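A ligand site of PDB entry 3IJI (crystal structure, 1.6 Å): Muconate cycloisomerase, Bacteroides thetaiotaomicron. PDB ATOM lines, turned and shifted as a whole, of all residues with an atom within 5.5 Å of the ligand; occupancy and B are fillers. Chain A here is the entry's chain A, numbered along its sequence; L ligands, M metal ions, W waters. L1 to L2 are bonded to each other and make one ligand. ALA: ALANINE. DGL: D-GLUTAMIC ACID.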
ATOM      1  N   PHE A  16     -32.358 -18.435   6.853  1.00  0.00           N
ATOM      2  CA  PHE A  16     -31.637 -17.250   7.295  1.00  0.00           C
ATOM      3  C   PHE A  16     -30.655 -17.639   8.396  1.00  0.00           C
ATOM      4  O   PHE A  16     -31.044 -18.232   9.401  1.00  0.00           O
ATOM      5  CB  PHE A  16     -32.654 -16.225   7.817  1.00  0.00           C
ATOM      6  CG  PHE A  16     -32.047 -14.922   8.220  1.00  0.00           C
ATOM      7  CD1 PHE A  16     -31.535 -14.042   7.257  1.00  0.00           C
ATOM      8  CD2 PHE A  16     -31.971 -14.560   9.561  1.00  0.00           C
ATOM      9  CE1 PHE A  16     -30.961 -12.828   7.633  1.00  0.00           C
ATOM     10  CE2 PHE A  16     -31.409 -13.347   9.946  1.00  0.00           C
ATOM     11  CZ  PHE A  16     -30.896 -12.484   8.980  1.00  0.00           C
ATOM     12  N   VAL A  18     -27.461 -16.690  11.208  1.00  0.00           N
ATOM     13  CA  VAL A  18     -26.765 -15.746  12.073  1.00  0.00           C
ATOM     14  C   VAL A  18     -25.684 -16.596  12.733  1.00  0.00           C
ATOM     15  O   VAL A  18     -25.990 -17.456  13.571  1.00  0.00           O
ATOM     16  CB  VAL A  18     -27.694 -15.179  13.164  1.00  0.00           C
ATOM     17  CG1 VAL A  18     -26.952 -14.148  14.002  1.00  0.00           C
ATOM     18  CG2 VAL A  18     -28.933 -14.552  12.522  1.00  0.00           C
ATOM     19  N   ARG A  23     -32.423 -20.507  10.568  1.00  0.00           N
ATOM     20  CA  ARG A  23     -33.837 -20.627  10.882  1.00  0.00           C
ATOM     21  C   ARG A  23     -34.687 -20.268   9.667  1.00  0.00           C
ATOM     22  O   ARG A  23     -34.203 -19.666   8.714  1.00  0.00           O
ATOM     23  CB  ARG A  23     -34.206 -19.738  12.069  1.00  0.00           C
ATOM     24  CG  ARG A  23     -34.282 -18.237  11.788  1.00  0.00           C
ATOM     25  CD  ARG A  23     -34.653 -17.508  13.076  1.00  0.00           C
ATOM     26  NE  ARG A  23     -35.052 -16.107  12.872  1.00  0.00           N
ATOM     27  CZ  ARG A  23     -34.229 -15.070  12.896  1.00  0.00           C
ATOM     28  NH1 ARG A  23     -32.925 -15.241  13.105  1.00  0.00           N
ATOM     29  NH2 ARG A  23     -34.706 -13.847  12.728  1.00  0.00           N
ATOM     30  N   THR A  26     -39.619 -16.620  12.320  1.00  0.00           N
ATOM     31  CA  THR A  26     -39.258 -15.708  13.386  1.00  0.00           C
ATOM     32  C   THR A  26     -40.470 -15.368  14.245  1.00  0.00           C
ATOM     33  O   THR A  26     -41.476 -14.850  13.749  1.00  0.00           O
ATOM     34  CB  THR A  26     -38.694 -14.368  12.847  1.00  0.00           C
ATOM     35  OG1 THR A  26     -37.553 -14.629  12.030  1.00  0.00           O
ATOM     36  CG2 THR A  26     -38.286 -13.467  14.006  1.00  0.00           C
ATOM     37  N   PRO A  47     -36.007 -12.801  17.384  1.00  0.00           N
ATOM     38  CA  PRO A  47     -35.103 -13.857  16.896  1.00  0.00           C
ATOM     39  C   PRO A  47     -34.808 -14.676  18.155  1.00  0.00           C
ATOM     40  O   PRO A  47     -34.375 -14.129  19.169  1.00  0.00           O
ATOM     41  CB  PRO A  47     -33.885 -13.059  16.416  1.00  0.00           C
ATOM     42  CG  PRO A  47     -34.519 -11.784  15.912  1.00  0.00           C
ATOM     43  CD  PRO A  47     -35.536 -11.467  16.991  1.00  0.00           C
ATOM     44  N   TYR A  49     -32.411 -16.423  19.465  1.00  0.00           N
ATOM     45  CA  TYR A  49     -31.166 -16.252  20.209  1.00  0.00           C
ATOM     46  C   TYR A  49     -31.056 -14.943  20.984  1.00  0.00           C
ATOM     47  O   TYR A  49     -30.097 -14.739  21.730  1.00  0.00           O
ATOM     48  CB  TYR A  49     -29.978 -16.395  19.246  1.00  0.00           C
ATOM     49  CG  TYR A  49     -29.930 -15.329  18.183  1.00  0.00           C
ATOM     50  CD1 TYR A  49     -29.290 -14.123  18.423  1.00  0.00           C
ATOM     51  CD2 TYR A  49     -30.550 -15.528  16.947  1.00  0.00           C
ATOM     52  CE1 TYR A  49     -29.272 -13.115  17.449  1.00  0.00           C
ATOM     53  CE2 TYR A  49     -30.543 -14.539  15.978  1.00  0.00           C
ATOM     54  CZ  TYR A  49     -29.904 -13.332  16.240  1.00  0.00           C
ATOM     55  OH  TYR A  49     -29.898 -12.342  15.293  1.00  0.00           O
ATOM     56  N   THR A 129     -27.913  -8.260   2.011  1.00  0.00           N
ATOM     57  CA  THR A 129     -26.879  -9.256   2.249  1.00  0.00           C
ATOM     58  C   THR A 129     -26.648 -10.310   1.177  1.00  0.00           C
ATOM     59  O   THR A 129     -27.592 -10.815   0.560  1.00  0.00           O
ATOM     60  CB  THR A 129     -27.151  -9.983   3.581  1.00  0.00           C
ATOM     61  OG1 THR A 129     -27.178  -9.019   4.640  1.00  0.00           O
ATOM     62  CG2 THR A 129     -26.065 -11.014   3.878  1.00  0.00           C
ATOM     63  N   LYS A 153     -24.043  -5.972   1.969  1.00  0.00           N
ATOM     64  CA  LYS A 153     -23.593  -6.395   3.287  1.00  0.00           C
ATOM     65  C   LYS A 153     -23.085  -7.831   3.219  1.00  0.00           C
ATOM     66  O   LYS A 153     -23.656  -8.670   2.521  1.00  0.00           O
ATOM     67  CB  LYS A 153     -24.735  -6.314   4.296  1.00  0.00           C
ATOM     68  CG  LYS A 153     -24.361  -6.850   5.678  1.00  0.00           C
ATOM     69  CD  LYS A 153     -25.502  -6.669   6.662  1.00  0.00           C
ATOM     70  CE  LYS A 153     -25.142  -7.222   8.036  1.00  0.00           C
ATOM     71  NZ  LYS A 153     -26.224  -6.953   9.021  1.00  0.00           N
ATOM     72  N   LYS A 155     -21.621 -10.872   5.909  1.00  0.00           N
ATOM     73  CA  LYS A 155     -21.422 -11.293   7.290  1.00  0.00           C
ATOM     74  C   LYS A 155     -20.182 -12.168   7.366  1.00  0.00           C
ATOM     75  O   LYS A 155     -20.213 -13.356   7.002  1.00  0.00           O
ATOM     76  CB  LYS A 155     -22.662 -12.045   7.775  1.00  0.00           C
ATOM     77  CG  LYS A 155     -23.899 -11.154   7.797  1.00  0.00           C
ATOM     78  CD  LYS A 155     -25.201 -11.949   7.896  1.00  0.00           C
ATOM     79  CE  LYS A 155     -26.392 -11.005   7.804  1.00  0.00           C
ATOM     80  NZ  LYS A 155     -27.696 -11.718   7.723  1.00  0.00           N
ATOM     81  N   ASP A 179     -19.964  -7.111   8.565  1.00  0.00           N
ATOM     82  CA  ASP A 179     -20.330  -7.309   9.956  1.00  0.00           C
ATOM     83  C   ASP A 179     -19.593  -8.589  10.370  1.00  0.00           C
ATOM     84  O   ASP A 179     -19.945  -9.683   9.931  1.00  0.00           O
ATOM     85  CB  ASP A 179     -21.835  -7.512  10.116  1.00  0.00           C
ATOM     86  CG  ASP A 179     -22.259  -7.529  11.574  1.00  0.00           C
ATOM     87  OD1 ASP A 179     -21.402  -7.822  12.422  1.00  0.00           O
ATOM     88  OD2 ASP A 179     -23.446  -7.253  11.855  1.00  0.00           O
ATOM     89  N   ASN A 181     -19.485  -9.821  13.315  1.00  0.00           N
ATOM     90  CA  ASN A 181     -20.226 -10.512  14.351  1.00  0.00           C
ATOM     91  C   ASN A 181     -19.309 -11.097  15.432  1.00  0.00           C
ATOM     92  O   ASN A 181     -19.423 -12.276  15.769  1.00  0.00           O
ATOM     93  CB  ASN A 181     -21.063 -11.644  13.727  1.00  0.00           C
ATOM     94  CG  ASN A 181     -22.209 -11.113  12.884  1.00  0.00           C
ATOM     95  OD1 ASN A 181     -23.162 -10.543  13.418  1.00  0.00           O
ATOM     96  ND2 ASN A 181     -22.119 -11.298  11.572  1.00  0.00           N
ATOM     97  N   GLU A 206     -18.244  -3.587  11.172  1.00  0.00           N
ATOM     98  CA  GLU A 206     -19.162  -3.686  12.300  1.00  0.00           C
ATOM     99  C   GLU A 206     -18.757  -4.810  13.256  1.00  0.00           C
ATOM    100  O   GLU A 206     -18.457  -5.924  12.832  1.00  0.00           O
ATOM    101  CB  GLU A 206     -20.585  -3.913  11.778  1.00  0.00           C
ATOM    102  CG  GLU A 206     -21.659  -4.089  12.843  1.00  0.00           C
ATOM    103  CD  GLU A 206     -23.047  -4.265  12.238  1.00  0.00           C
ATOM    104  OE1 GLU A 206     -23.973  -4.646  12.977  1.00  0.00           O
ATOM    105  OE2 GLU A 206     -23.215  -4.001  11.025  1.00  0.00           O
ATOM    106  N   ASP A 231     -22.283  -3.108  17.742  1.00  0.00           N
ATOM    107  CA  ASP A 231     -23.616  -3.714  17.657  1.00  0.00           C
ATOM    108  C   ASP A 231     -23.848  -4.512  18.933  1.00  0.00           C
ATOM    109  O   ASP A 231     -24.514  -4.050  19.851  1.00  0.00           O
ATOM    110  CB  ASP A 231     -23.711  -4.635  16.429  1.00  0.00           C
ATOM    111  CG  ASP A 231     -25.120  -5.159  16.220  1.00  0.00           C
ATOM    112  OD1 ASP A 231     -25.967  -4.989  17.125  1.00  0.00           O
ATOM    113  OD2 ASP A 231     -25.393  -5.738  15.138  1.00  0.00           O
ATOM    114  N   GLU A 232     -23.295  -5.721  19.003  1.00  0.00           N
ATOM    115  CA  GLU A 232     -23.451  -6.555  20.194  1.00  0.00           C
ATOM    116  C   GLU A 232     -22.891  -5.856  21.435  1.00  0.00           C
ATOM    117  O   GLU A 232     -23.263  -6.185  22.561  1.00  0.00           O
ATOM    118  CB  GLU A 232     -22.747  -7.905  20.002  1.00  0.00           C
ATOM    119  CG  GLU A 232     -23.447  -8.896  19.077  1.00  0.00           C
ATOM    120  CD  GLU A 232     -23.578  -8.383  17.651  1.00  0.00           C
ATOM    121  OE1 GLU A 232     -22.601  -7.815  17.130  1.00  0.00           O
ATOM    122  OE2 GLU A 232     -24.659  -8.570  17.053  1.00  0.00           O
ATOM    123  N   ASN A 251     -24.691   1.014  16.470  1.00  0.00           N
ATOM    124  CA  ASN A 251     -25.772   0.472  15.672  1.00  0.00           C
ATOM    125  C   ASN A 251     -27.001   0.417  16.566  1.00  0.00           C
ATOM    126  O   ASN A 251     -26.952  -0.126  17.664  1.00  0.00           O
ATOM    127  CB  ASN A 251     -25.424  -0.943  15.189  1.00  0.00           C
ATOM    128  CG  ASN A 251     -26.426  -1.478  14.182  1.00  0.00           C
ATOM    129  OD1 ASN A 251     -27.490  -0.893  13.971  1.00  0.00           O
ATOM    130  ND2 ASN A 251     -26.106  -2.608  13.562  1.00  0.00           N
ATOM    131  N   LYS A 253     -31.055  -0.709  17.038  1.00  0.00           N
ATOM    132  CA  LYS A 253     -32.124  -1.580  16.568  1.00  0.00           C
ATOM    133  C   LYS A 253     -33.281  -1.428  17.550  1.00  0.00           C
ATOM    134  O   LYS A 253     -33.102  -1.539  18.761  1.00  0.00           O
ATOM    135  CB  LYS A 253     -31.657  -3.043  16.523  1.00  0.00           C
ATOM    136  CG  LYS A 253     -30.449  -3.262  15.615  1.00  0.00           C
ATOM    137  CD  LYS A 253     -30.008  -4.724  15.618  1.00  0.00           C
ATOM    138  CE  LYS A 253     -28.617  -4.863  15.003  1.00  0.00           C
ATOM    139  NZ  LYS A 253     -28.089  -6.255  15.108  1.00  0.00           N
ATOM    140  N   CYS A 281     -31.887  -3.945  11.872  1.00  0.00           N
ATOM    141  CA  CYS A 281     -33.201  -4.535  12.101  1.00  0.00           C
ATOM    142  C   CYS A 281     -33.116  -6.053  12.194  1.00  0.00           C
ATOM    143  O   CYS A 281     -32.084  -6.657  11.926  1.00  0.00           O
ATOM    144  CB  CYS A 281     -34.133  -4.199  10.938  1.00  0.00           C
ATOM    145  SG  CYS A 281     -33.650  -4.983   9.366  1.00  0.00           S
ATOM    146  N   MET A 282     -34.233  -6.653  12.601  1.00  0.00           N
ATOM    147  CA  MET A 282     -34.345  -8.108  12.665  1.00  0.00           C
ATOM    148  C   MET A 282     -35.272  -8.397  11.483  1.00  0.00           C
ATOM    149  O   MET A 282     -35.725  -7.471  10.816  1.00  0.00           O
ATOM    150  CB  MET A 282     -35.075  -8.556  13.936  1.00  0.00           C
ATOM    151  CG  MET A 282     -34.612  -7.911  15.204  1.00  0.00           C
ATOM    152  SD  MET A 282     -32.902  -8.239  15.514  1.00  0.00           S
ATOM    153  CE  MET A 282     -32.637  -7.191  16.936  1.00  0.00           C
ATOM    154  N   THR A 283     -35.550  -9.671  11.215  1.00  0.00           N
ATOM    155  CA  THR A 283     -36.505  -9.986  10.164  1.00  0.00           C
ATOM    156  C   THR A 283     -37.782  -9.413  10.794  1.00  0.00           C
ATOM    157  O   THR A 283     -38.154  -9.810  11.907  1.00  0.00           O
ATOM    158  CB  THR A 283     -36.641 -11.498   9.980  1.00  0.00           C
ATOM    159  OG1 THR A 283     -36.910 -12.112  11.246  1.00  0.00           O
ATOM    160  CG2 THR A 283     -35.345 -12.078   9.418  1.00  0.00           C
ATOM    161  N   ASP A 303     -29.205  -0.862   7.581  1.00  0.00           N
ATOM    162  CA  ASP A 303     -29.458  -2.222   7.154  1.00  0.00           C
ATOM    163  C   ASP A 303     -30.935  -2.374   7.509  1.00  0.00           C
ATOM    164  O   ASP A 303     -31.286  -2.884   8.568  1.00  0.00           O
ATOM    165  CB  ASP A 303     -28.601  -3.221   7.939  1.00  0.00           C
ATOM    166  CG  ASP A 303     -28.670  -4.630   7.378  1.00  0.00           C
ATOM    167  OD1 ASP A 303     -28.544  -4.776   6.141  1.00  0.00           O
ATOM    168  OD2 ASP A 303     -28.831  -5.584   8.160  1.00  0.00           O
ATOM    169  N   ASP A 305     -33.651  -3.929   5.589  1.00  0.00           N
ATOM    170  CA  ASP A 305     -34.229  -4.799   4.566  1.00  0.00           C
ATOM    171  C   ASP A 305     -35.021  -5.949   5.179  1.00  0.00           C
ATOM    172  O   ASP A 305     -35.399  -6.880   4.476  1.00  0.00           O
ATOM    173  CB  ASP A 305     -33.108  -5.369   3.706  1.00  0.00           C
ATOM    174  CG  ASP A 305     -32.173  -6.287   4.501  1.00  0.00           C
ATOM    175  OD1 ASP A 305     -32.232  -6.247   5.743  1.00  0.00           O
ATOM    176  OD2 ASP A 305     -31.381  -7.029   3.880  1.00  0.00           O
ATOM    177  N   GLY A 306     -35.274  -5.881   6.479  1.00  0.00           N
ATOM    178  CA  GLY A 306     -35.978  -6.946   7.174  1.00  0.00           C
ATOM    179  C   GLY A 306     -37.261  -7.480   6.570  1.00  0.00           C
ATOM    180  O   GLY A 306     -37.503  -8.695   6.578  1.00  0.00           O
ATOM    181  N   LEU A 309     -37.171  -9.929   3.566  1.00  0.00           N
ATOM    182  CA  LEU A 309     -36.764 -11.286   3.879  1.00  0.00           C
ATOM    183  C   LEU A 309     -37.908 -12.202   4.302  1.00  0.00           C
ATOM    184  O   LEU A 309     -37.709 -13.402   4.490  1.00  0.00           O
ATOM    185  CB  LEU A 309     -35.697 -11.254   4.968  1.00  0.00           C
ATOM    186  CG  LEU A 309     -34.532 -10.297   4.695  1.00  0.00           C
ATOM    187  CD1 LEU A 309     -33.550 -10.350   5.854  1.00  0.00           C
ATOM    188  CD2 LEU A 309     -33.840 -10.686   3.400  1.00  0.00           C
HETATM  189  N   ALA L   1     -30.609  -7.536   7.237  1.00  0.00           N
HETATM  190  CA  ALA L   1     -30.958  -7.857   8.624  1.00  0.00           C
HETATM  191  C   ALA L   1     -29.909  -8.661   9.415  1.00  0.00           C
HETATM  192  O   ALA L   1     -28.947  -9.177   8.847  1.00  0.00           O
HETATM  193  CB  ALA L   1     -32.266  -8.613   8.645  1.00  0.00           C
HETATM  194  N   DGL L   2     -30.104  -8.755  10.734  1.00  0.00           N
HETATM  195  CA  DGL L   2     -29.185  -9.515  11.598  1.00  0.00           C
HETATM  196  C   DGL L   2     -28.430  -8.631  12.617  1.00  0.00           C
HETATM  197  O   DGL L   2     -27.673  -9.211  13.419  1.00  0.00           O
HETATM  198  CB  DGL L   2     -29.932 -10.656  12.314  1.00  0.00           C
HETATM  199  CG  DGL L   2     -31.322 -10.319  12.880  1.00  0.00           C
HETATM  200  CD  DGL L   2     -32.222 -11.534  13.009  1.00  0.00           C
HETATM  201  OE1 DGL L   2     -31.780 -12.567  13.562  1.00  0.00           O
HETATM  202  OE2 DGL L   2     -33.381 -11.445  12.564  1.00  0.00           O
HETATM  203  OXT DGL L   2     -28.584  -7.388  12.598  1.00  0.00           O
HETATM  204 MG    MG M   1     -24.425  -6.520  13.547  1.00  0.00          MG
HETATM  205  O   HOH W   1     -29.751 -10.075   5.813  1.00  0.00           O
HETATM  206  O   HOH W   2     -26.071  -6.263  12.397  1.00  0.00           O
HETATM  207  O   HOH W   3     -29.421  -5.335  10.841  1.00  0.00           O
HETATM  208  O   HOH W   4     -28.771  -6.998   4.734  1.00  0.00           O
HETATM  209  O   HOH W   5     -25.127  -8.360  14.143  1.00  0.00           O
HETATM  210  O   HOH W   6     -26.223 -11.143  11.775  1.00  0.00           O
HETATM  211  O   HOH W   7     -28.513 -10.205  15.826  1.00  0.00           O
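OE1 of DGL L2 sits at hydrogen-bond distance from OH of Tyr 49 (2.6 Å). NZ of Lys 155 is in hydrogen-bond range of O of ALA L1 (3.0 Å). An oxygen (OE2) of DGL L2 lies within salt-bridge range of the guanidinium group (NH2) of Arg 23. A nitrogen (N) of ALA L1 lies within salt-bridge range of the side-chain carboxylate of Asp 303, 2.8 Å away. OD1 of Asp 305 lies within salt-bridge range of N of ALA L1, at 2.6 Å. NZ of Lys 253 lies within salt-bridge range of OXT of DGL L2, at 2.8 Å. The backbone NH of Thr 283 sits at hydrogen-bond distance from an oxygen (OE2) of DGL L2 (3.1 Å). The backbone carbonyl oxygen (O) of Cys 281 is in hydrogen-bond range of a nitrogen (N) of DGL L2 (3.1 Å).
The side-chain hydroxyl (OG1) of Thr 26 is in hydrogen-bond range of the guanidinium group (NE) of Arg 23. NZ of Lys 253 is in salt-bridge range of OD1 of Asp 231 (3.2 Å). The backbone carbonyl oxygen (O) of Arg 23 lies within hydrogen-bond range of the backbone NH (N) of Phe 16 (2.9 Å). The backbone carbonyl oxygen (O) of Asp 303 is in hydrogen-bond range of the side-chain sulfur (SG) of Cys 281 (3.3 Å). The side-chain hydroxyl (OG1) of Thr 283 lies within hydrogen-bond range of the side-chain hydroxyl (OG1) of Thr 26 (2.7 Å). The side-chain amino group of Lys 153 lies close to the side-chain carboxylate of Asp 179. SG of Cys 281 sits at hydrogen-bond distance from N of Gly 306 (3.4 Å). OD2 of Asp 303 lies within salt-bridge range of NZ of Lys 153, 3.1 Å away.
Merely in contact with the ligand: Phe 16, Val 18, Pro 47, Lys 153, Met 282 and Leu 309. Hydrophobic or aromatic side chains that line the ligand: Phe 16, Val 18, Pro 47, Tyr 49, Met 282 and Leu 309. Along chain A the residues within 4 Å of the ligand span positions 16 to 309.
Water W7 bridges OH of Tyr 49 and O of DGL L2. Water W2 lies within hydrogen-bond range of an oxygen (OXT) of DGL L2 (2.8 Å), the side-chain amino group (NZ) of Lys 253 (3.4 Å) and the side-chain amino group (NZ) of Lys 153 (3.4 Å). Water W5 lies within hydrogen-bond range of O of DGL L2 (2.8 Å), OE2 of Glu 232 (3.0 Å) and OD1 of Asn 181 (3.0 Å). Water W3 lies within hydrogen-bond range of OD2 of Asp 303 (2.8 Å), OXT of DGL L2 (2.8 Å) and N of Cys 281 (3.0 Å). Water W1 lies within hydrogen-bond range of OG1 of Thr 129, N of ALA L1 and NZ of Lys 155. Water W4 lies within hydrogen-bond range of the side-chain hydroxyl (OG1) of Thr 129 (2.6 Å), the side-chain carboxylate (OD1) of Asp 303 (2.6 Å), the side-chain carboxylate (OD2) of Asp 305 (2.7 Å) and a nitrogen (N) of ALA L1 (3.2 Å).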
